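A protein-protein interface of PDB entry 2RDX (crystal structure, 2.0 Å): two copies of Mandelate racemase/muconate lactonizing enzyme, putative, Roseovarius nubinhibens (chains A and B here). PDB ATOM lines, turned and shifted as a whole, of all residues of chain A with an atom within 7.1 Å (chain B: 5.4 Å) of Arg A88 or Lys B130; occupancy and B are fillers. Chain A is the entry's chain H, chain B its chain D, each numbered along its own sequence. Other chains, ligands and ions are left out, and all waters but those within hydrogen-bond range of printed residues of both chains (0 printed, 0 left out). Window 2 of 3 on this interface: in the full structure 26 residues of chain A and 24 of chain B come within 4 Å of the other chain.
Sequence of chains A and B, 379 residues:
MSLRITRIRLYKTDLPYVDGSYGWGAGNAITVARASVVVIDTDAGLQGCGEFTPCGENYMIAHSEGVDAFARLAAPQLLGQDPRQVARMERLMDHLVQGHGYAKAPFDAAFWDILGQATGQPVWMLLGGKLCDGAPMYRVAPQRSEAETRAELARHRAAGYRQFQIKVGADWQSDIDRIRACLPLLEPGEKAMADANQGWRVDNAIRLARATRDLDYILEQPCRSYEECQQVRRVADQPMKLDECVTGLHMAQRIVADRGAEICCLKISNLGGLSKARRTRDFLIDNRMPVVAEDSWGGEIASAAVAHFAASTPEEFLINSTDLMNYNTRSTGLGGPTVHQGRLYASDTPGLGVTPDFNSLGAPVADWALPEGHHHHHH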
ATOM      1  N   LEU A  78      -6.848  17.923  35.742  1.00  0.00           N
ATOM      2  CA  LEU A  78      -6.623  18.695  34.514  1.00  0.00           C
ATOM      3  C   LEU A  78      -6.416  17.814  33.295  1.00  0.00           C
ATOM      4  O   LEU A  78      -6.540  18.278  32.168  1.00  0.00           O
ATOM      5  CB  LEU A  78      -5.434  19.652  34.665  1.00  0.00           C
ATOM      6  CG  LEU A  78      -5.626  20.865  35.583  1.00  0.00           C
ATOM      7  CD1 LEU A  78      -4.321  21.610  35.739  1.00  0.00           C
ATOM      8  CD2 LEU A  78      -6.702  21.799  35.057  1.00  0.00           C
ATOM      9  N   GLN A  81      -8.629  17.504  29.667  1.00  0.00           N
ATOM     10  CA  GLN A  81      -9.292  18.780  29.441  1.00  0.00           C
ATOM     11  C   GLN A  81      -8.711  19.433  28.201  1.00  0.00           C
ATOM     12  O   GLN A  81      -7.641  19.045  27.748  1.00  0.00           O
ATOM     13  CB  GLN A  81      -9.071  19.701  30.634  1.00  0.00           C
ATOM     14  CG  GLN A  81      -9.755  19.272  31.921  1.00  0.00           C
ATOM     15  CD  GLN A  81     -11.258  19.489  31.887  1.00  0.00           C
ATOM     16  OE1 GLN A  81     -11.740  20.577  31.578  1.00  0.00           O
ATOM     17  NE2 GLN A  81     -12.004  18.451  32.208  1.00  0.00           N
ATOM     18  N   ASP A  82      -9.421  20.427  27.670  1.00  0.00           N
ATOM     19  CA  ASP A  82      -9.002  21.188  26.488  1.00  0.00           C
ATOM     20  C   ASP A  82      -8.190  22.416  26.909  1.00  0.00           C
ATOM     21  O   ASP A  82      -8.757  23.407  27.358  1.00  0.00           O
ATOM     22  CB  ASP A  82     -10.246  21.608  25.696  1.00  0.00           C
ATOM     23  CG  ASP A  82      -9.921  22.256  24.364  1.00  0.00           C
ATOM     24  OD1 ASP A  82      -8.747  22.582  24.100  1.00  0.00           O
ATOM     25  OD2 ASP A  82     -10.863  22.442  23.561  1.00  0.00           O
ATOM     26  N   ARG A  84      -6.610  24.770  25.286  1.00  0.00           N
ATOM     27  CA  ARG A  84      -6.704  26.025  24.547  1.00  0.00           C
ATOM     28  C   ARG A  84      -7.885  26.910  24.962  1.00  0.00           C
ATOM     29  O   ARG A  84      -7.934  28.089  24.617  1.00  0.00           O
ATOM     30  CB  ARG A  84      -6.613  25.793  23.035  1.00  0.00           C
ATOM     31  CG  ARG A  84      -7.727  25.016  22.400  1.00  0.00           C
ATOM     32  CD  ARG A  84      -7.151  23.957  21.481  1.00  0.00           C
ATOM     33  NE  ARG A  84      -7.918  23.723  20.259  1.00  0.00           N
ATOM     34  CZ  ARG A  84      -9.016  22.976  20.166  1.00  0.00           C
ATOM     35  NH1 ARG A  84      -9.535  22.390  21.232  1.00  0.00           N
ATOM     36  NH2 ARG A  84      -9.612  22.828  18.992  1.00  0.00           N
ATOM     37  N   GLN A  85      -8.812  26.354  25.737  1.00  0.00           N
ATOM     38  CA  GLN A  85      -9.869  27.151  26.345  1.00  0.00           C
ATOM     39  C   GLN A  85      -9.362  27.702  27.677  1.00  0.00           C
ATOM     40  O   GLN A  85      -9.719  27.195  28.749  1.00  0.00           O
ATOM     41  CB  GLN A  85     -11.142  26.315  26.523  1.00  0.00           C
ATOM     42  CG  GLN A  85     -11.527  25.574  25.259  1.00  0.00           C
ATOM     43  CD  GLN A  85     -12.941  25.058  25.271  1.00  0.00           C
ATOM     44  OE1 GLN A  85     -13.807  25.604  25.943  1.00  0.00           O
ATOM     45  NE2 GLN A  85     -13.188  24.002  24.498  1.00  0.00           N
ATOM     46  N   VAL A  86      -8.533  28.749  27.585  1.00  0.00           N
ATOM     47  CA  VAL A  86      -7.768  29.303  28.718  1.00  0.00           C
ATOM     48  C   VAL A  86      -8.613  29.751  29.906  1.00  0.00           C
ATOM     49  O   VAL A  86      -8.178  29.656  31.050  1.00  0.00           O
ATOM     50  CB  VAL A  86      -6.823  30.476  28.289  1.00  0.00           C
ATOM     51  CG1 VAL A  86      -5.768  29.978  27.324  1.00  0.00           C
ATOM     52  CG2 VAL A  86      -7.601  31.650  27.676  1.00  0.00           C
ATOM     53  N   ALA A  87      -9.822  30.224  29.623  1.00  0.00           N
ATOM     54  CA  ALA A  87     -10.698  30.747  30.657  1.00  0.00           C
ATOM     55  C   ALA A  87     -11.579  29.646  31.233  1.00  0.00           C
ATOM     56  O   ALA A  87     -12.153  29.811  32.309  1.00  0.00           O
ATOM     57  CB  ALA A  87     -11.525  31.908  30.121  1.00  0.00           C
ATOM     58  N   ARG A  88     -11.685  28.525  30.520  1.00  0.00           N
ATOM     59  CA  ARG A  88     -12.275  27.330  31.104  1.00  0.00           C
ATOM     60  C   ARG A  88     -11.266  26.716  32.076  1.00  0.00           C
ATOM     61  O   ARG A  88     -11.617  26.372  33.206  1.00  0.00           O
ATOM     62  CB  ARG A  88     -12.712  26.324  30.032  1.00  0.00           C
ATOM     63  CG  ARG A  88     -13.625  25.222  30.575  1.00  0.00           C
ATOM     64  CD  ARG A  88     -13.695  24.016  29.648  1.00  0.00           C
ATOM     65  NE  ARG A  88     -14.900  24.032  28.826  1.00  0.00           N
ATOM     66  CZ  ARG A  88     -15.124  23.214  27.801  1.00  0.00           C
ATOM     67  NH1 ARG A  88     -14.220  22.306  27.453  1.00  0.00           N
ATOM     68  NH2 ARG A  88     -16.253  23.309  27.116  1.00  0.00           N
ATOM     69  N   MET A  89     -10.007  26.635  31.641  1.00  0.00           N
ATOM     70  CA  MET A  89      -8.910  26.137  32.483  1.00  0.00           C
ATOM     71  C   MET A  89      -8.688  27.010  33.714  1.00  0.00           C
ATOM     72  O   MET A  89      -8.440  26.487  34.802  1.00  0.00           O
ATOM     73  CB  MET A  89      -7.610  25.975  31.678  1.00  0.00           C
ATOM     74  CG  MET A  89      -7.662  24.970  30.521  1.00  0.00           C
ATOM     75  SD  MET A  89      -8.029  23.249  30.970  1.00  0.00           S
ATOM     76  CE  MET A  89      -9.786  23.217  30.610  1.00  0.00           C
ATOM     77  N   GLU A  90      -8.803  28.330  33.532  1.00  0.00           N
ATOM     78  CA  GLU A  90      -8.722  29.302  34.626  1.00  0.00           C
ATOM     79  C   GLU A  90      -9.751  29.050  35.725  1.00  0.00           C
ATOM     80  O   GLU A  90      -9.390  28.943  36.903  1.00  0.00           O
ATOM     81  CB  GLU A  90      -8.881  30.730  34.096  1.00  0.00           C
ATOM     82  CG  GLU A  90      -8.855  31.783  35.199  1.00  0.00           C
ATOM     83  CD  GLU A  90      -9.029  33.188  34.711  1.00  0.00           C
ATOM     84  OE1 GLU A  90      -9.287  33.402  33.507  1.00  0.00           O
ATOM     85  OE2 GLU A  90      -8.909  34.092  35.558  1.00  0.00           O
ATOM     86  N   ARG A  91     -10.994  28.947  35.337  1.00  0.00           N
ATOM     87  CA  ARG A  91     -12.037  28.732  36.272  1.00  0.00           C
ATOM     88  C   ARG A  91     -12.149  27.345  36.855  1.00  0.00           C
ATOM     89  O   ARG A  91     -12.683  27.150  37.908  1.00  0.00           O
ATOM     90  CB  ARG A  91     -13.333  29.325  35.746  1.00  0.00           C
ATOM     91  CG  ARG A  91     -14.334  28.419  35.082  1.00  0.00           C
ATOM     92  CD  ARG A  91     -15.655  28.473  35.840  1.00  0.00           C
ATOM     93  NE  ARG A  91     -16.879  28.557  35.042  1.00  0.00           N
ATOM     94  CZ  ARG A  91     -17.177  27.781  34.010  1.00  0.00           C
ATOM     95  NH1 ARG A  91     -18.325  27.932  33.379  1.00  0.00           N
ATOM     96  NH2 ARG A  91     -16.322  26.866  33.601  1.00  0.00           N
ATOM     97  N   LEU A  92     -11.572  26.380  36.161  1.00  0.00           N
ATOM     98  CA  LEU A  92     -11.430  25.027  36.685  1.00  0.00           C
ATOM     99  C   LEU A  92     -10.357  25.002  37.772  1.00  0.00           C
ATOM    100  O   LEU A  92     -10.596  24.456  38.847  1.00  0.00           O
ATOM    101  CB  LEU A  92     -11.096  24.016  35.587  1.00  0.00           C
ATOM    102  CG  LEU A  92     -10.893  22.543  35.980  1.00  0.00           C
ATOM    103  CD1 LEU A  92     -12.107  21.940  36.708  1.00  0.00           C
ATOM    104  CD2 LEU A  92     -10.554  21.728  34.742  1.00  0.00           C
ATOM    105  N   MET A  93      -9.188  25.587  37.489  1.00  0.00           N
ATOM    106  CA  MET A  93      -8.120  25.703  38.489  1.00  0.00           C
ATOM    107  C   MET A  93      -8.597  26.493  39.713  1.00  0.00           C
ATOM    108  O   MET A  93      -8.275  26.143  40.848  1.00  0.00           O
ATOM    109  CB  MET A  93      -6.840  26.308  37.881  1.00  0.00           C
ATOM    110  CG  MET A  93      -5.995  25.308  37.049  1.00  0.00           C
ATOM    111  SD  MET A  93      -4.365  25.846  36.470  1.00  0.00           S
ATOM    112  CE  MET A  93      -4.735  27.385  35.638  1.00  0.00           C
ATOM    113  N   ASP A  94      -9.405  27.527  39.474  1.00  0.00           N
ATOM    114  CA  ASP A  94      -9.964  28.341  40.543  1.00  0.00           C
ATOM    115  C   ASP A  94     -11.103  27.648  41.299  1.00  0.00           C
ATOM    116  O   ASP A  94     -11.395  28.011  42.434  1.00  0.00           O
ATOM    117  CB  ASP A  94     -10.426  29.700  40.010  1.00  0.00           C
ATOM    118  CG  ASP A  94      -9.269  30.647  39.719  1.00  0.00           C
ATOM    119  OD1 ASP A  94      -8.101  30.279  39.971  1.00  0.00           O
ATOM    120  OD2 ASP A  94      -9.530  31.780  39.249  1.00  0.00           O
ATOM    121  N   TRP B 124     -15.748  32.567  20.052  1.00  0.00           N
ATOM    122  CA  TRP B 124     -15.809  32.177  21.475  1.00  0.00           C
ATOM    123  C   TRP B 124     -14.502  31.592  22.029  1.00  0.00           C
ATOM    124  O   TRP B 124     -14.189  31.805  23.198  1.00  0.00           O
ATOM    125  CB  TRP B 124     -17.001  31.242  21.806  1.00  0.00           C
ATOM    126  CG  TRP B 124     -17.074  29.888  21.099  1.00  0.00           C
ATOM    127  CD1 TRP B 124     -17.910  29.556  20.069  1.00  0.00           C
ATOM    128  CD2 TRP B 124     -16.331  28.683  21.404  1.00  0.00           C
ATOM    129  NE1 TRP B 124     -17.721  28.246  19.700  1.00  0.00           N
ATOM    130  CE2 TRP B 124     -16.768  27.686  20.508  1.00  0.00           C
ATOM    131  CE3 TRP B 124     -15.349  28.354  22.347  1.00  0.00           C
ATOM    132  CZ2 TRP B 124     -16.239  26.387  20.515  1.00  0.00           C
ATOM    133  CZ3 TRP B 124     -14.823  27.069  22.351  1.00  0.00           C
ATOM    134  CH2 TRP B 124     -15.272  26.101  21.445  1.00  0.00           C
ATOM    135  N   GLY B 128     -12.006  33.166  25.169  1.00  0.00           N
ATOM    136  CA  GLY B 128     -11.616  32.425  26.371  1.00  0.00           C
ATOM    137  C   GLY B 128     -12.013  30.958  26.429  1.00  0.00           C
ATOM    138  O   GLY B 128     -11.437  30.194  27.198  1.00  0.00           O
ATOM    139  N   GLY B 129     -12.998  30.564  25.622  1.00  0.00           N
ATOM    140  CA  GLY B 129     -13.503  29.186  25.624  1.00  0.00           C
ATOM    141  C   GLY B 129     -15.018  29.097  25.714  1.00  0.00           C
ATOM    142  O   GLY B 129     -15.700  30.118  25.819  1.00  0.00           O
ATOM    143  N   LYS B 130     -15.542  27.873  25.649  1.00  0.00           N
ATOM    144  CA  LYS B 130     -16.976  27.648  25.753  1.00  0.00           C
ATOM    145  C   LYS B 130     -17.328  27.455  27.212  1.00  0.00           C
ATOM    146  O   LYS B 130     -17.270  26.345  27.743  1.00  0.00           O
ATOM    147  CB  LYS B 130     -17.430  26.440  24.926  1.00  0.00           C
ATOM    148  CG  LYS B 130     -18.946  26.326  24.832  1.00  0.00           C
ATOM    149  CD  LYS B 130     -19.374  25.418  23.717  1.00  0.00           C
ATOM    150  CE  LYS B 130     -19.424  26.158  22.401  1.00  0.00           C
ATOM    151  NZ  LYS B 130     -19.715  25.222  21.294  1.00  0.00           N
ATOM    152  N   LEU B 131     -17.701  28.559  27.845  1.00  0.00           N
ATOM    153  CA  LEU B 131     -17.914  28.613  29.284  1.00  0.00           C
ATOM    154  C   LEU B 131     -19.387  28.422  29.610  1.00  0.00           C
ATOM    155  O   LEU B 131     -19.764  28.160  30.750  1.00  0.00           O
ATOM    156  CB  LEU B 131     -17.386  29.940  29.814  1.00  0.00           C
ATOM    157  CG  LEU B 131     -15.949  29.965  30.343  1.00  0.00           C
ATOM    158  CD1 LEU B 131     -14.920  29.436  29.368  1.00  0.00           C
ATOM    159  CD2 LEU B 131     -15.598  31.367  30.733  1.00  0.00           C
ATOM    160  N   CYS B 132     -20.207  28.543  28.575  1.00  0.00           N
ATOM    161  CA  CYS B 132     -21.621  28.249  28.644  1.00  0.00           C
ATOM    162  C   CYS B 132     -22.007  27.559  27.346  1.00  0.00           C
ATOM    163  O   CYS B 132     -22.003  28.180  26.285  1.00  0.00           O
ATOM    164  CB  CYS B 132     -22.416  29.546  28.796  1.00  0.00           C
ATOM    165  SG  CYS B 132     -24.192  29.305  28.977  1.00  0.00           S
ATOM    166  N   ASP B 133     -22.319  26.275  27.420  1.00  0.00           N
ATOM    167  CA  ASP B 133     -22.832  25.576  26.251  1.00  0.00           C
ATOM    168  C   ASP B 133     -24.348  25.760  26.245  1.00  0.00           C
ATOM    169  O   ASP B 133     -25.081  25.057  26.944  1.00  0.00           O
ATOM    170  CB  ASP B 133     -22.418  24.097  26.257  1.00  0.00           C
ATOM    171  CG  ASP B 133     -22.416  23.463  24.857  1.00  0.00           C
ATOM    172  OD1 ASP B 133     -22.573  24.180  23.844  1.00  0.00           O
ATOM    173  OD2 ASP B 133     -22.244  22.226  24.773  1.00  0.00           O
ATOM    174  N   ALA B 311     -21.494  32.664  24.890  1.00  0.00           N
ATOM    175  CA  ALA B 311     -20.855  31.356  25.046  1.00  0.00           C
ATOM    176  C   ALA B 311     -19.559  31.427  25.843  1.00  0.00           C
ATOM    177  O   ALA B 311     -19.115  30.427  26.387  1.00  0.00           O
ATOM    178  CB  ALA B 311     -20.595  30.717  23.676  1.00  0.00           C
ATOM    179  N   SER B 312     -18.939  32.601  25.891  1.00  0.00           N
ATOM    180  CA  SER B 312     -17.701  32.760  26.646  1.00  0.00           C
ATOM    181  C   SER B 312     -17.932  33.427  27.992  1.00  0.00           C
ATOM    182  O   SER B 312     -16.990  33.914  28.620  1.00  0.00           O
ATOM    183  CB  SER B 312     -16.659  33.523  25.822  1.00  0.00           C
ATOM    184  OG  SER B 312     -17.186  34.734  25.307  1.00  0.00           O
ATOM    185  N   ALA B 346     -23.870  29.318  19.932  1.00  0.00           N
ATOM    186  CA  ALA B 346     -22.938  29.924  18.988  1.00  0.00           C
ATOM    187  C   ALA B 346     -22.496  28.889  17.955  1.00  0.00           C
ATOM    188  O   ALA B 346     -22.755  27.693  18.121  1.00  0.00           O
ATOM    189  CB  ALA B 346     -21.729  30.486  19.730  1.00  0.00           C
ATOM    190  N   ASP B 348     -19.489  26.844  15.775  1.00  0.00           N
ATOM    191  CA  ASP B 348     -18.195  26.283  16.153  1.00  0.00           C
ATOM    192  C   ASP B 348     -17.168  26.300  15.022  1.00  0.00           C
ATOM    193  O   ASP B 348     -16.011  25.927  15.219  1.00  0.00           O
ATOM    194  CB  ASP B 348     -18.378  24.886  16.757  1.00  0.00           C
ATOM    195  CG  ASP B 348     -19.206  24.911  18.031  1.00  0.00           C
ATOM    196  OD1 ASP B 348     -19.069  25.877  18.823  1.00  0.00           O
ATOM    197  OD2 ASP B 348     -20.004  23.976  18.236  1.00  0.00           O
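The backbone NH of Lys B130 is in hydrogen-bond range of the side-chain amide oxygen of Gln A85, 2.9 Å away. The backbone carbonyl oxygen of Gly B128 sits at hydrogen-bond distance from the backbone NH of Val A86, at 3.3 Å. O of Gly B128 lies within hydrogen-bond range of N of Ala A87, 2.9 Å away. The backbone carbonyl oxygen of Lys B130 sits at hydrogen-bond distance from the guanidinium group of Arg A88, at 3.3 Å. NH1 of Arg A91 sits at hydrogen-bond distance from O of Leu B131 (3.0 Å).
The side-chain amino group (NZ) of Lys B130 is in salt-bridge range of the side-chain carboxylate (OD1) of Asp B348 (2.6 Å). The side-chain amide nitrogen (NE2) of Gln A85 lies within hydrogen-bond range of the side-chain carboxylate (OD2) of Asp A82, at 3.0 Å. O of Trp B124 is in hydrogen-bond range of N of Gly B129. The backbone NH (N) of Leu B131 lies within hydrogen-bond range of the backbone carbonyl oxygen (O) of Ala B311 (2.8 Å). OD1 of Asp B133 is in salt-bridge range of NZ of Lys B130 (3.97 Å). The side-chain amide oxygen (OE1) of Gln A85 sits close to the guanidinium group (NE) of Arg A88 (3.5 Å).
Gln A85 touches Gly B128. OE1 of Gln A85 touches CA of Gly B129 (3.6 Å). Ala A87 touches Leu B131. Arg A88 touches Gly B128 (N to O, 3.7 Å). CD1 of Leu B131 touches N of Arg A88, 3.6 Å away.
Of the printed residues of chain B, Ala A87 touches Gly B128 (2.9 Å) and Leu B131 (3.8 Å). Of chain B, only Gly B128 (3.7 Å), Lys B130 (3.3 Å) and Leu B131 (3.6 Å) come within 4 Å of Arg A88. Met A89 touches none of the printed residues of chain B. Of the printed residues of chain A, Gly B128 touches Gln A85, Val A86, Ala A87 and Arg A88. Lys B130 touches just these residues of chain A: Gln A85 and Arg A88. The nearest printed residue of chain A that does not touch Lys B130 is Arg A91 (5.9 Å). The nearest printed residue of chain B that does not touch Ala A87 is Gly B129 (4.9 Å).
Printed residues of chain B that touch a printed residue of chain A: Gly B128, Gly B129, Lys B130 and Leu B131. Among the printed residues, 10 pairs touch across the chains.
No position is printed for both chains.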
